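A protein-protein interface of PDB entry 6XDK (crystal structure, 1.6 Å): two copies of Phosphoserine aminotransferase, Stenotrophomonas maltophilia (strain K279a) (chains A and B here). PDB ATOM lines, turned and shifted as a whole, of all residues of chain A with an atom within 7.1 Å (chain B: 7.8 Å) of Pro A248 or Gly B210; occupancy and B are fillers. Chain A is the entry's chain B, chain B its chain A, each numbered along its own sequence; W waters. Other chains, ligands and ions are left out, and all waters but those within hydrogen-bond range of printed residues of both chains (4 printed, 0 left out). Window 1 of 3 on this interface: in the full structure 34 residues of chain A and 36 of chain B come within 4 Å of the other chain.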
ATOM      1  N   ILE A  44      17.277  21.104  14.473  1.00  0.00           N
ATOM      2  CA  ILE A  44      18.705  20.871  14.324  1.00  0.00           C
ATOM      3  C   ILE A  44      19.343  22.034  13.576  1.00  0.00           C
ATOM      4  O   ILE A  44      20.469  22.443  13.880  1.00  0.00           O
ATOM      5  CB  ILE A  44      18.950  19.531  13.604  1.00  0.00           C
ATOM      6  CG1 ILE A  44      18.759  18.361  14.567  1.00  0.00           C
ATOM      7  CG2 ILE A  44      20.339  19.483  13.062  1.00  0.00           C
ATOM      8  CD1 ILE A  44      20.057  17.982  15.329  1.00  0.00           C
ATOM      9  N   VAL A  45      18.609  22.605  12.612  1.00  0.00           N
ATOM     10  CA  VAL A  45      19.149  23.665  11.760  1.00  0.00           C
ATOM     11  C   VAL A  45      19.583  24.867  12.592  1.00  0.00           C
ATOM     12  O   VAL A  45      20.584  25.525  12.278  1.00  0.00           O
ATOM     13  CB  VAL A  45      18.117  24.075  10.681  1.00  0.00           C
ATOM     14  CG1 VAL A  45      18.563  25.360   9.995  1.00  0.00           C
ATOM     15  CG2 VAL A  45      17.892  22.952   9.656  1.00  0.00           C
ATOM     16  N   HIS A  49      26.600  25.069  17.175  1.00  0.00           N
ATOM     17  CA  HIS A  49      27.633  24.038  17.099  1.00  0.00           C
ATOM     18  C   HIS A  49      28.276  23.782  18.456  1.00  0.00           C
ATOM     19  O   HIS A  49      28.788  22.679  18.699  1.00  0.00           O
ATOM     20  CB  HIS A  49      28.729  24.434  16.106  1.00  0.00           C
ATOM     21  CG  HIS A  49      28.378  24.206  14.663  1.00  0.00           C
ATOM     22  ND1 HIS A  49      27.675  25.127  13.915  1.00  0.00           N
ATOM     23  CD2 HIS A  49      28.676  23.187  13.820  1.00  0.00           C
ATOM     24  CE1 HIS A  49      27.541  24.682  12.679  1.00  0.00           C
ATOM     25  NE2 HIS A  49      28.133  23.503  12.595  1.00  0.00           N
ATOM     26  N   PHE A  54      24.012  19.822  20.170  1.00  0.00           N
ATOM     27  CA  PHE A  54      24.714  19.486  18.943  1.00  0.00           C
ATOM     28  C   PHE A  54      26.046  18.814  19.226  1.00  0.00           C
ATOM     29  O   PHE A  54      26.475  17.954  18.445  1.00  0.00           O
ATOM     30  CB  PHE A  54      24.952  20.695  18.046  1.00  0.00           C
ATOM     31  CG  PHE A  54      25.607  20.295  16.768  1.00  0.00           C
ATOM     32  CD1 PHE A  54      24.873  19.600  15.814  1.00  0.00           C
ATOM     33  CD2 PHE A  54      26.970  20.475  16.567  1.00  0.00           C
ATOM     34  CE1 PHE A  54      25.485  19.136  14.637  1.00  0.00           C
ATOM     35  CE2 PHE A  54      27.583  20.024  15.389  1.00  0.00           C
ATOM     36  CZ  PHE A  54      26.836  19.361  14.435  1.00  0.00           C
ATOM     37  N   SER A  81      33.717  20.934   5.166  1.00  0.00           N
ATOM     38  CA  SER A  81      33.032  21.488   4.006  1.00  0.00           C
ATOM     39  C   SER A  81      33.991  21.535   2.814  1.00  0.00           C
ATOM     40  O   SER A  81      35.206  21.352   2.945  1.00  0.00           O
ATOM     41  CB  SER A  81      32.502  22.879   4.333  1.00  0.00           C
ATOM     42  OG  SER A  81      33.571  23.735   4.679  1.00  0.00           O
ATOM     43  N   VAL A 209      24.773  15.414   1.630  1.00  0.00           N
ATOM     44  CA  VAL A 209      25.017  16.792   1.204  1.00  0.00           C
ATOM     45  C   VAL A 209      25.845  17.601   2.202  1.00  0.00           C
ATOM     46  O   VAL A 209      25.514  17.671   3.391  1.00  0.00           O
ATOM     47  CB  VAL A 209      23.675  17.491   0.916  1.00  0.00           C
ATOM     48  CG1 VAL A 209      22.758  17.419   2.115  1.00  0.00           C
ATOM     49  CG2 VAL A 209      23.903  18.935   0.495  1.00  0.00           C
ATOM     50  N   GLY A 210      26.944  18.192   1.724  1.00  0.00           N
ATOM     51  CA  GLY A 210      27.768  19.093   2.516  1.00  0.00           C
ATOM     52  C   GLY A 210      28.730  18.475   3.516  1.00  0.00           C
ATOM     53  O   GLY A 210      29.342  19.219   4.291  1.00  0.00           O
ATOM     54  N   VAL A 211      28.887  17.157   3.547  1.00  0.00           N
ATOM     55  CA  VAL A 211      29.721  16.497   4.549  1.00  0.00           C
ATOM     56  C   VAL A 211      30.820  15.710   3.844  1.00  0.00           C
ATOM     57  O   VAL A 211      30.548  14.630   3.310  1.00  0.00           O
ATOM     58  CB  VAL A 211      28.882  15.570   5.450  1.00  0.00           C
ATOM     59  CG1 VAL A 211      29.795  14.872   6.470  1.00  0.00           C
ATOM     60  CG2 VAL A 211      27.728  16.364   6.148  1.00  0.00           C
ATOM     61  N   THR A 246      33.657  23.139   9.425  1.00  0.00           N
ATOM     62  CA  THR A 246      32.742  22.032   9.645  1.00  0.00           C
ATOM     63  C   THR A 246      31.419  22.293   8.947  1.00  0.00           C
ATOM     64  O   THR A 246      31.007  23.448   8.782  1.00  0.00           O
ATOM     65  CB  THR A 246      32.474  21.819  11.139  1.00  0.00           C
ATOM     66  OG1 THR A 246      31.822  22.974  11.676  1.00  0.00           O
ATOM     67  CG2 THR A 246      33.780  21.543  11.905  1.00  0.00           C
ATOM     68  N   PRO A 247      30.751  21.223   8.544  1.00  0.00           N
ATOM     69  CA  PRO A 247      29.462  21.369   7.903  1.00  0.00           C
ATOM     70  C   PRO A 247      28.478  22.074   8.821  1.00  0.00           C
ATOM     71  O   PRO A 247      28.674  22.155  10.046  1.00  0.00           O
ATOM     72  CB  PRO A 247      29.036  19.923   7.627  1.00  0.00           C
ATOM     73  CG  PRO A 247      30.387  19.161   7.536  1.00  0.00           C
ATOM     74  CD  PRO A 247      31.183  19.814   8.624  1.00  0.00           C
ATOM     75  N   PRO A 248      27.444  22.630   8.253  1.00  0.00           N
ATOM     76  CA  PRO A 248      26.282  23.053   9.047  1.00  0.00           C
ATOM     77  C   PRO A 248      25.787  21.923   9.926  1.00  0.00           C
ATOM     78  O   PRO A 248      26.023  20.750   9.628  1.00  0.00           O
ATOM     79  CB  PRO A 248      25.253  23.427   7.967  1.00  0.00           C
ATOM     80  CG  PRO A 248      26.108  23.797   6.800  1.00  0.00           C
ATOM     81  CD  PRO A 248      27.230  22.834   6.811  1.00  0.00           C
ATOM     82  N   THR A 249      25.059  22.266  10.992  1.00  0.00           N
ATOM     83  CA  THR A 249      24.644  21.243  11.942  1.00  0.00           C
ATOM     84  C   THR A 249      23.702  20.238  11.307  1.00  0.00           C
ATOM     85  O   THR A 249      23.785  19.042  11.606  1.00  0.00           O
ATOM     86  CB  THR A 249      23.974  21.887  13.144  1.00  0.00           C
ATOM     87  OG1 THR A 249      22.938  22.751  12.669  1.00  0.00           O
ATOM     88  CG2 THR A 249      24.967  22.670  13.944  1.00  0.00           C
ATOM     89  N   TRP A 250      22.775  20.694  10.454  1.00  0.00           N
ATOM     90  CA  TRP A 250      21.784  19.757   9.930  1.00  0.00           C
ATOM     91  C   TRP A 250      22.451  18.763   8.990  1.00  0.00           C
ATOM     92  O   TRP A 250      22.132  17.573   9.013  1.00  0.00           O
ATOM     93  CB  TRP A 250      20.623  20.503   9.248  1.00  0.00           C
ATOM     94  CG  TRP A 250      19.455  19.585   8.895  1.00  0.00           C
ATOM     95  CD1 TRP A 250      18.454  19.159   9.722  1.00  0.00           C
ATOM     96  CD2 TRP A 250      19.209  18.978   7.625  1.00  0.00           C
ATOM     97  NE1 TRP A 250      17.604  18.309   9.041  1.00  0.00           N
ATOM     98  CE2 TRP A 250      18.050  18.184   7.752  1.00  0.00           C
ATOM     99  CE3 TRP A 250      19.886  18.998   6.402  1.00  0.00           C
ATOM    100  CZ2 TRP A 250      17.522  17.456   6.688  1.00  0.00           C
ATOM    101  CZ3 TRP A 250      19.366  18.272   5.349  1.00  0.00           C
ATOM    102  CH2 TRP A 250      18.196  17.507   5.498  1.00  0.00           C
ATOM    103  N   ASN A 251      23.424  19.227   8.206  1.00  0.00           N
ATOM    104  CA  ASN A 251      24.185  18.336   7.335  1.00  0.00           C
ATOM    105  C   ASN A 251      24.953  17.302   8.147  1.00  0.00           C
ATOM    106  O   ASN A 251      24.944  16.099   7.824  1.00  0.00           O
ATOM    107  CB  ASN A 251      25.146  19.161   6.488  1.00  0.00           C
ATOM    108  CG  ASN A 251      24.435  20.230   5.709  1.00  0.00           C
ATOM    109  OD1 ASN A 251      23.811  21.156   6.284  1.00  0.00           O
ATOM    110  ND2 ASN A 251      24.445  20.086   4.391  1.00  0.00           N
ATOM    111  N   TRP A 252      25.635  17.761   9.195  1.00  0.00           N
ATOM    112  CA  TRP A 252      26.370  16.855  10.070  1.00  0.00           C
ATOM    113  C   TRP A 252      25.417  15.873  10.741  1.00  0.00           C
ATOM    114  O   TRP A 252      25.699  14.672  10.832  1.00  0.00           O
ATOM    115  CB  TRP A 252      27.126  17.695  11.091  1.00  0.00           C
ATOM    116  CG  TRP A 252      28.276  17.080  11.689  1.00  0.00           C
ATOM    117  CD1 TRP A 252      28.524  15.748  11.819  1.00  0.00           C
ATOM    118  CD2 TRP A 252      29.370  17.762  12.307  1.00  0.00           C
ATOM    119  NE1 TRP A 252      29.710  15.554  12.494  1.00  0.00           N
ATOM    120  CE2 TRP A 252      30.250  16.776  12.797  1.00  0.00           C
ATOM    121  CE3 TRP A 252      29.696  19.112  12.471  1.00  0.00           C
ATOM    122  CZ2 TRP A 252      31.442  17.097  13.448  1.00  0.00           C
ATOM    123  CZ3 TRP A 252      30.855  19.434  13.133  1.00  0.00           C
ATOM    124  CH2 TRP A 252      31.726  18.434  13.602  1.00  0.00           C
ATOM    125  N   TYR A 253      24.266  16.363  11.180  1.00  0.00           N
ATOM    126  CA  TYR A 253      23.257  15.473  11.745  1.00  0.00           C
ATOM    127  C   TYR A 253      22.775  14.452  10.723  1.00  0.00           C
ATOM    128  O   TYR A 253      22.608  13.269  11.048  1.00  0.00           O
ATOM    129  CB  TYR A 253      22.093  16.321  12.260  1.00  0.00           C
ATOM    130  CG  TYR A 253      20.736  15.680  12.248  1.00  0.00           C
ATOM    131  CD1 TYR A 253      20.286  14.958  13.332  1.00  0.00           C
ATOM    132  CD2 TYR A 253      19.872  15.874  11.179  1.00  0.00           C
ATOM    133  CE1 TYR A 253      19.010  14.396  13.339  1.00  0.00           C
ATOM    134  CE2 TYR A 253      18.601  15.333  11.176  1.00  0.00           C
ATOM    135  CZ  TYR A 253      18.174  14.607  12.259  1.00  0.00           C
ATOM    136  OH  TYR A 253      16.911  14.069  12.246  1.00  0.00           O
ATOM    137  N   LEU A 254      22.571  14.879   9.479  1.00  0.00           N
ATOM    138  CA  LEU A 254      22.152  13.929   8.451  1.00  0.00           C
ATOM    139  C   LEU A 254      23.216  12.864   8.220  1.00  0.00           C
ATOM    140  O   LEU A 254      22.889  11.677   8.091  1.00  0.00           O
ATOM    141  CB  LEU A 254      21.828  14.662   7.149  1.00  0.00           C
ATOM    142  CG  LEU A 254      21.061  13.851   6.100  1.00  0.00           C
ATOM    143  CD1 LEU A 254      19.696  13.384   6.641  1.00  0.00           C
ATOM    144  CD2 LEU A 254      20.905  14.694   4.848  1.00  0.00           C
ATOM    145  N   LEU B  80      29.095  29.895  -1.888  1.00  0.00           N
ATOM    146  CA  LEU B  80      30.326  29.161  -1.559  1.00  0.00           C
ATOM    147  C   LEU B  80      30.232  28.376  -0.253  1.00  0.00           C
ATOM    148  O   LEU B  80      29.562  28.779   0.689  1.00  0.00           O
ATOM    149  CB  LEU B  80      31.488  30.141  -1.437  1.00  0.00           C
ATOM    150  CG  LEU B  80      31.811  30.885  -2.743  1.00  0.00           C
ATOM    151  CD1 LEU B  80      32.628  32.089  -2.417  1.00  0.00           C
ATOM    152  CD2 LEU B  80      32.547  30.003  -3.701  1.00  0.00           C
ATOM    153  N   SER B  81      30.952  27.253  -0.193  1.00  0.00           N
ATOM    154  CA  SER B  81      31.116  26.562   1.084  1.00  0.00           C
ATOM    155  C   SER B  81      32.307  27.152   1.859  1.00  0.00           C
ATOM    156  O   SER B  81      33.111  27.910   1.330  1.00  0.00           O
ATOM    157  CB  SER B  81      31.299  25.065   0.836  1.00  0.00           C
ATOM    158  OG  SER B  81      32.463  24.866   0.064  1.00  0.00           O
ATOM    159  N   GLY B  82      32.425  26.795   3.140  1.00  0.00           N
ATOM    160  CA  GLY B  82      33.613  27.153   3.916  1.00  0.00           C
ATOM    161  C   GLY B  82      33.511  28.384   4.808  1.00  0.00           C
ATOM    162  O   GLY B  82      34.466  28.683   5.539  1.00  0.00           O
ATOM    163  N   GLY B  83      32.405  29.095   4.786  1.00  0.00           N
ATOM    164  CA  GLY B  83      32.219  30.221   5.678  1.00  0.00           C
ATOM    165  C   GLY B  83      33.060  31.437   5.355  1.00  0.00           C
ATOM    166  O   GLY B  83      33.857  31.489   4.416  1.00  0.00           O
ATOM    167  N   GLY B 201      29.323  35.267   5.436  1.00  0.00           N
ATOM    168  CA  GLY B 201      29.092  33.911   5.873  1.00  0.00           C
ATOM    169  C   GLY B 201      27.674  33.731   6.413  1.00  0.00           C
ATOM    170  O   GLY B 201      26.939  34.683   6.668  1.00  0.00           O
ATOM    171  N   ALA B 202      27.299  32.471   6.614  1.00  0.00           N
ATOM    172  CA  ALA B 202      26.010  32.161   7.220  1.00  0.00           C
ATOM    173  C   ALA B 202      26.058  32.389   8.729  1.00  0.00           C
ATOM    174  O   ALA B 202      27.097  32.740   9.304  1.00  0.00           O
ATOM    175  CB  ALA B 202      25.621  30.719   6.928  1.00  0.00           C
ATOM    176  N   GLN B 203      24.910  32.169   9.371  1.00  0.00           N
ATOM    177  CA  GLN B 203      24.681  32.076  10.813  1.00  0.00           C
ATOM    178  C   GLN B 203      24.331  33.400  11.477  1.00  0.00           C
ATOM    179  O   GLN B 203      23.964  33.393  12.656  1.00  0.00           O
ATOM    180  CB  GLN B 203      25.856  31.447  11.582  1.00  0.00           C
ATOM    181  CG  GLN B 203      26.048  29.985  11.246  1.00  0.00           C
ATOM    182  CD  GLN B 203      25.498  29.072  12.312  1.00  0.00           C
ATOM    183  OE1 GLN B 203      25.769  29.239  13.514  1.00  0.00           O
ATOM    184  NE2 GLN B 203      24.702  28.098  11.884  1.00  0.00           N
ATOM    185  N   LEU B 206      22.009  36.287   7.663  1.00  0.00           N
ATOM    186  CA  LEU B 206      21.358  35.331   6.772  1.00  0.00           C
ATOM    187  C   LEU B 206      20.666  34.204   7.523  1.00  0.00           C
ATOM    188  O   LEU B 206      19.873  33.480   6.915  1.00  0.00           O
ATOM    189  CB  LEU B 206      22.372  34.720   5.791  1.00  0.00           C
ATOM    190  CG  LEU B 206      23.025  35.681   4.800  1.00  0.00           C
ATOM    191  CD1 LEU B 206      24.159  34.999   4.047  1.00  0.00           C
ATOM    192  CD2 LEU B 206      21.992  36.282   3.847  1.00  0.00           C
ATOM    193  N   GLY B 207      20.957  34.021   8.806  1.00  0.00           N
ATOM    194  CA  GLY B 207      20.464  32.869   9.520  1.00  0.00           C
ATOM    195  C   GLY B 207      21.307  31.649   9.180  1.00  0.00           C
ATOM    196  O   GLY B 207      22.239  31.709   8.361  1.00  0.00           O
ATOM    197  N   PRO B 208      21.005  30.528   9.811  1.00  0.00           N
ATOM    198  CA  PRO B 208      21.827  29.302   9.637  1.00  0.00           C
ATOM    199  C   PRO B 208      21.469  28.564   8.354  1.00  0.00           C
ATOM    200  O   PRO B 208      20.818  27.516   8.367  1.00  0.00           O
ATOM    201  CB  PRO B 208      21.493  28.506  10.900  1.00  0.00           C
ATOM    202  CG  PRO B 208      20.069  28.875  11.156  1.00  0.00           C
ATOM    203  CD  PRO B 208      19.996  30.344  10.867  1.00  0.00           C
ATOM    204  N   VAL B 209      21.870  29.163   7.229  1.00  0.00           N
ATOM    205  CA  VAL B 209      21.543  28.617   5.920  1.00  0.00           C
ATOM    206  C   VAL B 209      22.656  27.764   5.358  1.00  0.00           C
ATOM    207  O   VAL B 209      22.421  27.039   4.376  1.00  0.00           O
ATOM    208  CB  VAL B 209      21.175  29.705   4.890  1.00  0.00           C
ATOM    209  CG1 VAL B 209      19.868  30.401   5.281  1.00  0.00           C
ATOM    210  CG2 VAL B 209      22.298  30.707   4.673  1.00  0.00           C
ATOM    211  N   GLY B 210      23.852  27.816   5.937  1.00  0.00           N
ATOM    212  CA  GLY B 210      24.865  26.844   5.557  1.00  0.00           C
ATOM    213  C   GLY B 210      25.587  27.140   4.267  1.00  0.00           C
ATOM    214  O   GLY B 210      26.204  26.231   3.694  1.00  0.00           O
ATOM    215  N   VAL B 211      25.540  28.382   3.794  1.00  0.00           N
ATOM    216  CA  VAL B 211      26.256  28.794   2.590  1.00  0.00           C
ATOM    217  C   VAL B 211      26.691  30.237   2.775  1.00  0.00           C
ATOM    218  O   VAL B 211      26.025  31.017   3.466  1.00  0.00           O
ATOM    219  CB  VAL B 211      25.379  28.618   1.331  1.00  0.00           C
ATOM    220  CG1 VAL B 211      24.161  29.499   1.433  1.00  0.00           C
ATOM    221  CG2 VAL B 211      26.150  28.960   0.102  1.00  0.00           C
ATOM    222  N   ALA B 212      27.819  30.591   2.162  1.00  0.00           N
ATOM    223  CA  ALA B 212      28.337  31.957   2.153  1.00  0.00           C
ATOM    224  C   ALA B 212      28.061  32.586   0.799  1.00  0.00           C
ATOM    225  O   ALA B 212      27.988  31.886  -0.211  1.00  0.00           O
ATOM    226  CB  ALA B 212      29.840  31.959   2.413  1.00  0.00           C
ATOM    227  N   PRO B 248      26.864  22.680  -1.821  1.00  0.00           N
ATOM    228  CA  PRO B 248      25.908  22.213  -0.803  1.00  0.00           C
ATOM    229  C   PRO B 248      24.466  22.576  -1.155  1.00  0.00           C
ATOM    230  O   PRO B 248      23.953  23.633  -0.762  1.00  0.00           O
ATOM    231  CB  PRO B 248      26.396  22.922   0.469  1.00  0.00           C
ATOM    232  CG  PRO B 248      27.034  24.170  -0.035  1.00  0.00           C
ATOM    233  CD  PRO B 248      27.668  23.819  -1.357  1.00  0.00           C
ATOM    234  N   THR B 249      23.807  21.672  -1.878  1.00  0.00           N
ATOM    235  CA  THR B 249      22.538  21.956  -2.556  1.00  0.00           C
ATOM    236  C   THR B 249      21.421  22.375  -1.587  1.00  0.00           C
ATOM    237  O   THR B 249      20.807  23.431  -1.752  1.00  0.00           O
ATOM    238  CB  THR B 249      22.131  20.726  -3.360  1.00  0.00           C
ATOM    239  OG1 THR B 249      22.352  19.563  -2.557  1.00  0.00           O
ATOM    240  CG2 THR B 249      22.997  20.591  -4.637  1.00  0.00           C
ATOM    241  N   TRP B 250      21.077  21.503  -0.628  1.00  0.00           N
ATOM    242  CA  TRP B 250      20.102  21.810   0.415  1.00  0.00           C
ATOM    243  C   TRP B 250      20.310  23.199   1.015  1.00  0.00           C
ATOM    244  O   TRP B 250      19.337  23.937   1.252  1.00  0.00           O
ATOM    245  CB  TRP B 250      20.191  20.735   1.501  1.00  0.00           C
ATOM    246  CG  TRP B 250      19.466  21.089   2.743  1.00  0.00           C
ATOM    247  CD1 TRP B 250      20.014  21.571   3.898  1.00  0.00           C
ATOM    248  CD2 TRP B 250      18.060  21.031   2.958  1.00  0.00           C
ATOM    249  NE1 TRP B 250      19.032  21.794   4.821  1.00  0.00           N
ATOM    250  CE2 TRP B 250      17.825  21.471   4.269  1.00  0.00           C
ATOM    251  CE3 TRP B 250      16.975  20.637   2.170  1.00  0.00           C
ATOM    252  CZ2 TRP B 250      16.549  21.519   4.819  1.00  0.00           C
ATOM    253  CZ3 TRP B 250      15.720  20.687   2.707  1.00  0.00           C
ATOM    254  CH2 TRP B 250      15.510  21.131   4.019  1.00  0.00           C
ATOM    255  N   ASN B 251      21.575  23.566   1.265  1.00  0.00           N
ATOM    256  CA  ASN B 251      21.879  24.843   1.887  1.00  0.00           C
ATOM    257  C   ASN B 251      21.657  26.002   0.924  1.00  0.00           C
ATOM    258  O   ASN B 251      21.164  27.066   1.320  1.00  0.00           O
ATOM    259  CB  ASN B 251      23.310  24.825   2.415  1.00  0.00           C
ATOM    260  CG  ASN B 251      23.540  23.661   3.339  1.00  0.00           C
ATOM    261  OD1 ASN B 251      23.954  22.592   2.902  1.00  0.00           O
ATOM    262  ND2 ASN B 251      23.190  23.835   4.622  1.00  0.00           N
ATOM    263  N   TRP B 252      22.038  25.826  -0.339  1.00  0.00           N
ATOM    264  CA  TRP B 252      21.717  26.819  -1.359  1.00  0.00           C
ATOM    265  C   TRP B 252      20.204  27.029  -1.447  1.00  0.00           C
ATOM    266  O   TRP B 252      19.728  28.173  -1.494  1.00  0.00           O
ATOM    267  CB  TRP B 252      22.331  26.316  -2.667  1.00  0.00           C
ATOM    268  CG  TRP B 252      22.568  27.271  -3.720  1.00  0.00           C
ATOM    269  CD1 TRP B 252      21.945  28.481  -3.904  1.00  0.00           C
ATOM    270  CD2 TRP B 252      23.486  27.119  -4.806  1.00  0.00           C
ATOM    271  NE1 TRP B 252      22.415  29.078  -5.062  1.00  0.00           N
ATOM    272  CE2 TRP B 252      23.355  28.264  -5.631  1.00  0.00           C
ATOM    273  CE3 TRP B 252      24.410  26.139  -5.154  1.00  0.00           C
ATOM    274  CZ2 TRP B 252      24.121  28.453  -6.767  1.00  0.00           C
ATOM    275  CZ3 TRP B 252      25.146  26.318  -6.314  1.00  0.00           C
ATOM    276  CH2 TRP B 252      24.997  27.463  -7.097  1.00  0.00           C
ATOM    277  N   LEU B 254      17.991  26.475   1.034  1.00  0.00           N
ATOM    278  CA  LEU B 254      17.551  27.200   2.233  1.00  0.00           C
ATOM    279  C   LEU B 254      17.868  28.679   2.138  1.00  0.00           C
ATOM    280  O   LEU B 254      17.034  29.522   2.501  1.00  0.00           O
ATOM    281  CB  LEU B 254      18.205  26.641   3.496  1.00  0.00           C
ATOM    282  CG  LEU B 254      17.788  25.301   4.068  1.00  0.00           C
ATOM    283  CD1 LEU B 254      18.612  25.032   5.365  1.00  0.00           C
ATOM    284  CD2 LEU B 254      16.286  25.247   4.335  1.00  0.00           C
ATOM    285  N   ALA B 255      19.074  29.024   1.666  1.00  0.00           N
ATOM    286  CA  ALA B 255      19.401  30.426   1.446  1.00  0.00           C
ATOM    287  C   ALA B 255      18.413  31.065   0.480  1.00  0.00           C
ATOM    288  O   ALA B 255      17.957  32.194   0.691  1.00  0.00           O
ATOM    289  CB  ALA B 255      20.825  30.576   0.907  1.00  0.00           C
HETATM  290  O   HOH W   1      35.316  24.751   2.046  1.00  0.00           O
HETATM  291  O   HOH W   2      23.048  26.105  13.288  1.00  0.00           O
HETATM  292  O   HOH W   3      26.727  27.205  15.245  1.00  0.00           O
HETATM  293  O   HOH W   4      24.783  25.134  11.216  1.00  0.00           O
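Of the printed residues of chain B, Ser A81 touches Gly B82 (3.5 Å). Of chain B, only Gly B210 and Asn B251 come within 4 Å of Pro A248. Of chain A, only Pro A248 (3.5 Å) comes within 4 Å of Gly B210. Ala B212 touches none of the printed residues of chain A. Of the printed residues of chain A, Thr B249 touches Val A209. Printed residues of chain A within 4 Å of Asn B251: Pro A248 (3.6 Å) and Asn A251 (3.0 Å). The nearest residue of chain B that does not touch Pro A248 is Val B209 (5.5 Å). The nearest residue of chain A that does not touch Gly B210 is Asn A251 (5.8 Å).
The side-chain amide nitrogen of Asn B251 lies close to the backbone carbonyl oxygen of Val B209, at 3.3 Å. O of Val A209 is in hydrogen-bond range of ND2 of Asn A251, 2.8 Å away.
The side-chain amide oxygen (OD1) of Asn B251 sits at hydrogen-bond distance from the side-chain amide nitrogen (ND2) of Asn A251 (3.0 Å).
Of the 21 printed residues of chain B, 6 touch a printed residue of chain A. Printed residues of chain B that touch a printed residue of chain A: Gly B82, Pro B208, Gly B210, Thr B249, Trp B250 and Asn B251. Hydrophobic or aromatic side chains of chain B within 4 Å of the printed part of chain A: Pro B208 and Trp B250. Printed residues of chain A that touch a printed residue of chain B: Val A45, Ser A81, Val A209, Pro A248, Trp A250 and Asn A251. Hydrophobic or aromatic side chains of chain A that line the printed part of chain B: Val A45, Val A209, Pro A248 and Trp A250. Among the printed residues, no Asp or Glu carboxylate lies within 4 Å of a Lys or Arg side-chain nitrogen of the other chain.
Water W3 bridges ND1 of His A49 and OE1 of Gln B203. Water W2 lies within hydrogen-bond range of the backbone carbonyl oxygen of Val A45 (2.7 Å), the side-chain amide nitrogen of Gln B203 (2.9 Å) and the side-chain hydroxyl of Thr A249 (3.4 Å). Water W4 lies within hydrogen-bond range of N of Thr A249 (2.9 Å) and NE2 of Gln B203 (3.0 Å). Water W1 lies within hydrogen-bond range of OG of Ser A81 and OG of Ser B81.
Among the printed residues, merely in contact across the chains: Val A45 with Pro B208 (3.4 Å), Ser A81 with Gly B82 (3.5 Å), Val A209 with Thr B249 (3.5 Å), Val A209 with Trp B250 (3.98 Å), Pro A248 with Gly B210 (3.5 Å), Pro A248 with Asn B251 (3.6 Å) and Trp A250 with Trp B250 (3.3 Å).
Val A209 touches Thr B249, but with the chains exchanged Thr A249 does not touch Val B209 (8.2 Å). Pro A248 touches Gly B210, but with the chains exchanged Gly A210 does not touch Pro B248 (4.6 Å). Trp A250 touches its own counterpart, Trp B250. Asn B251 touches its own counterpart, Asn A251. 10 positions are printed for both chains. Of the 8 pairs that touch across the chains among the printed residues, 2 have their exchanged pair printed and touching as well.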
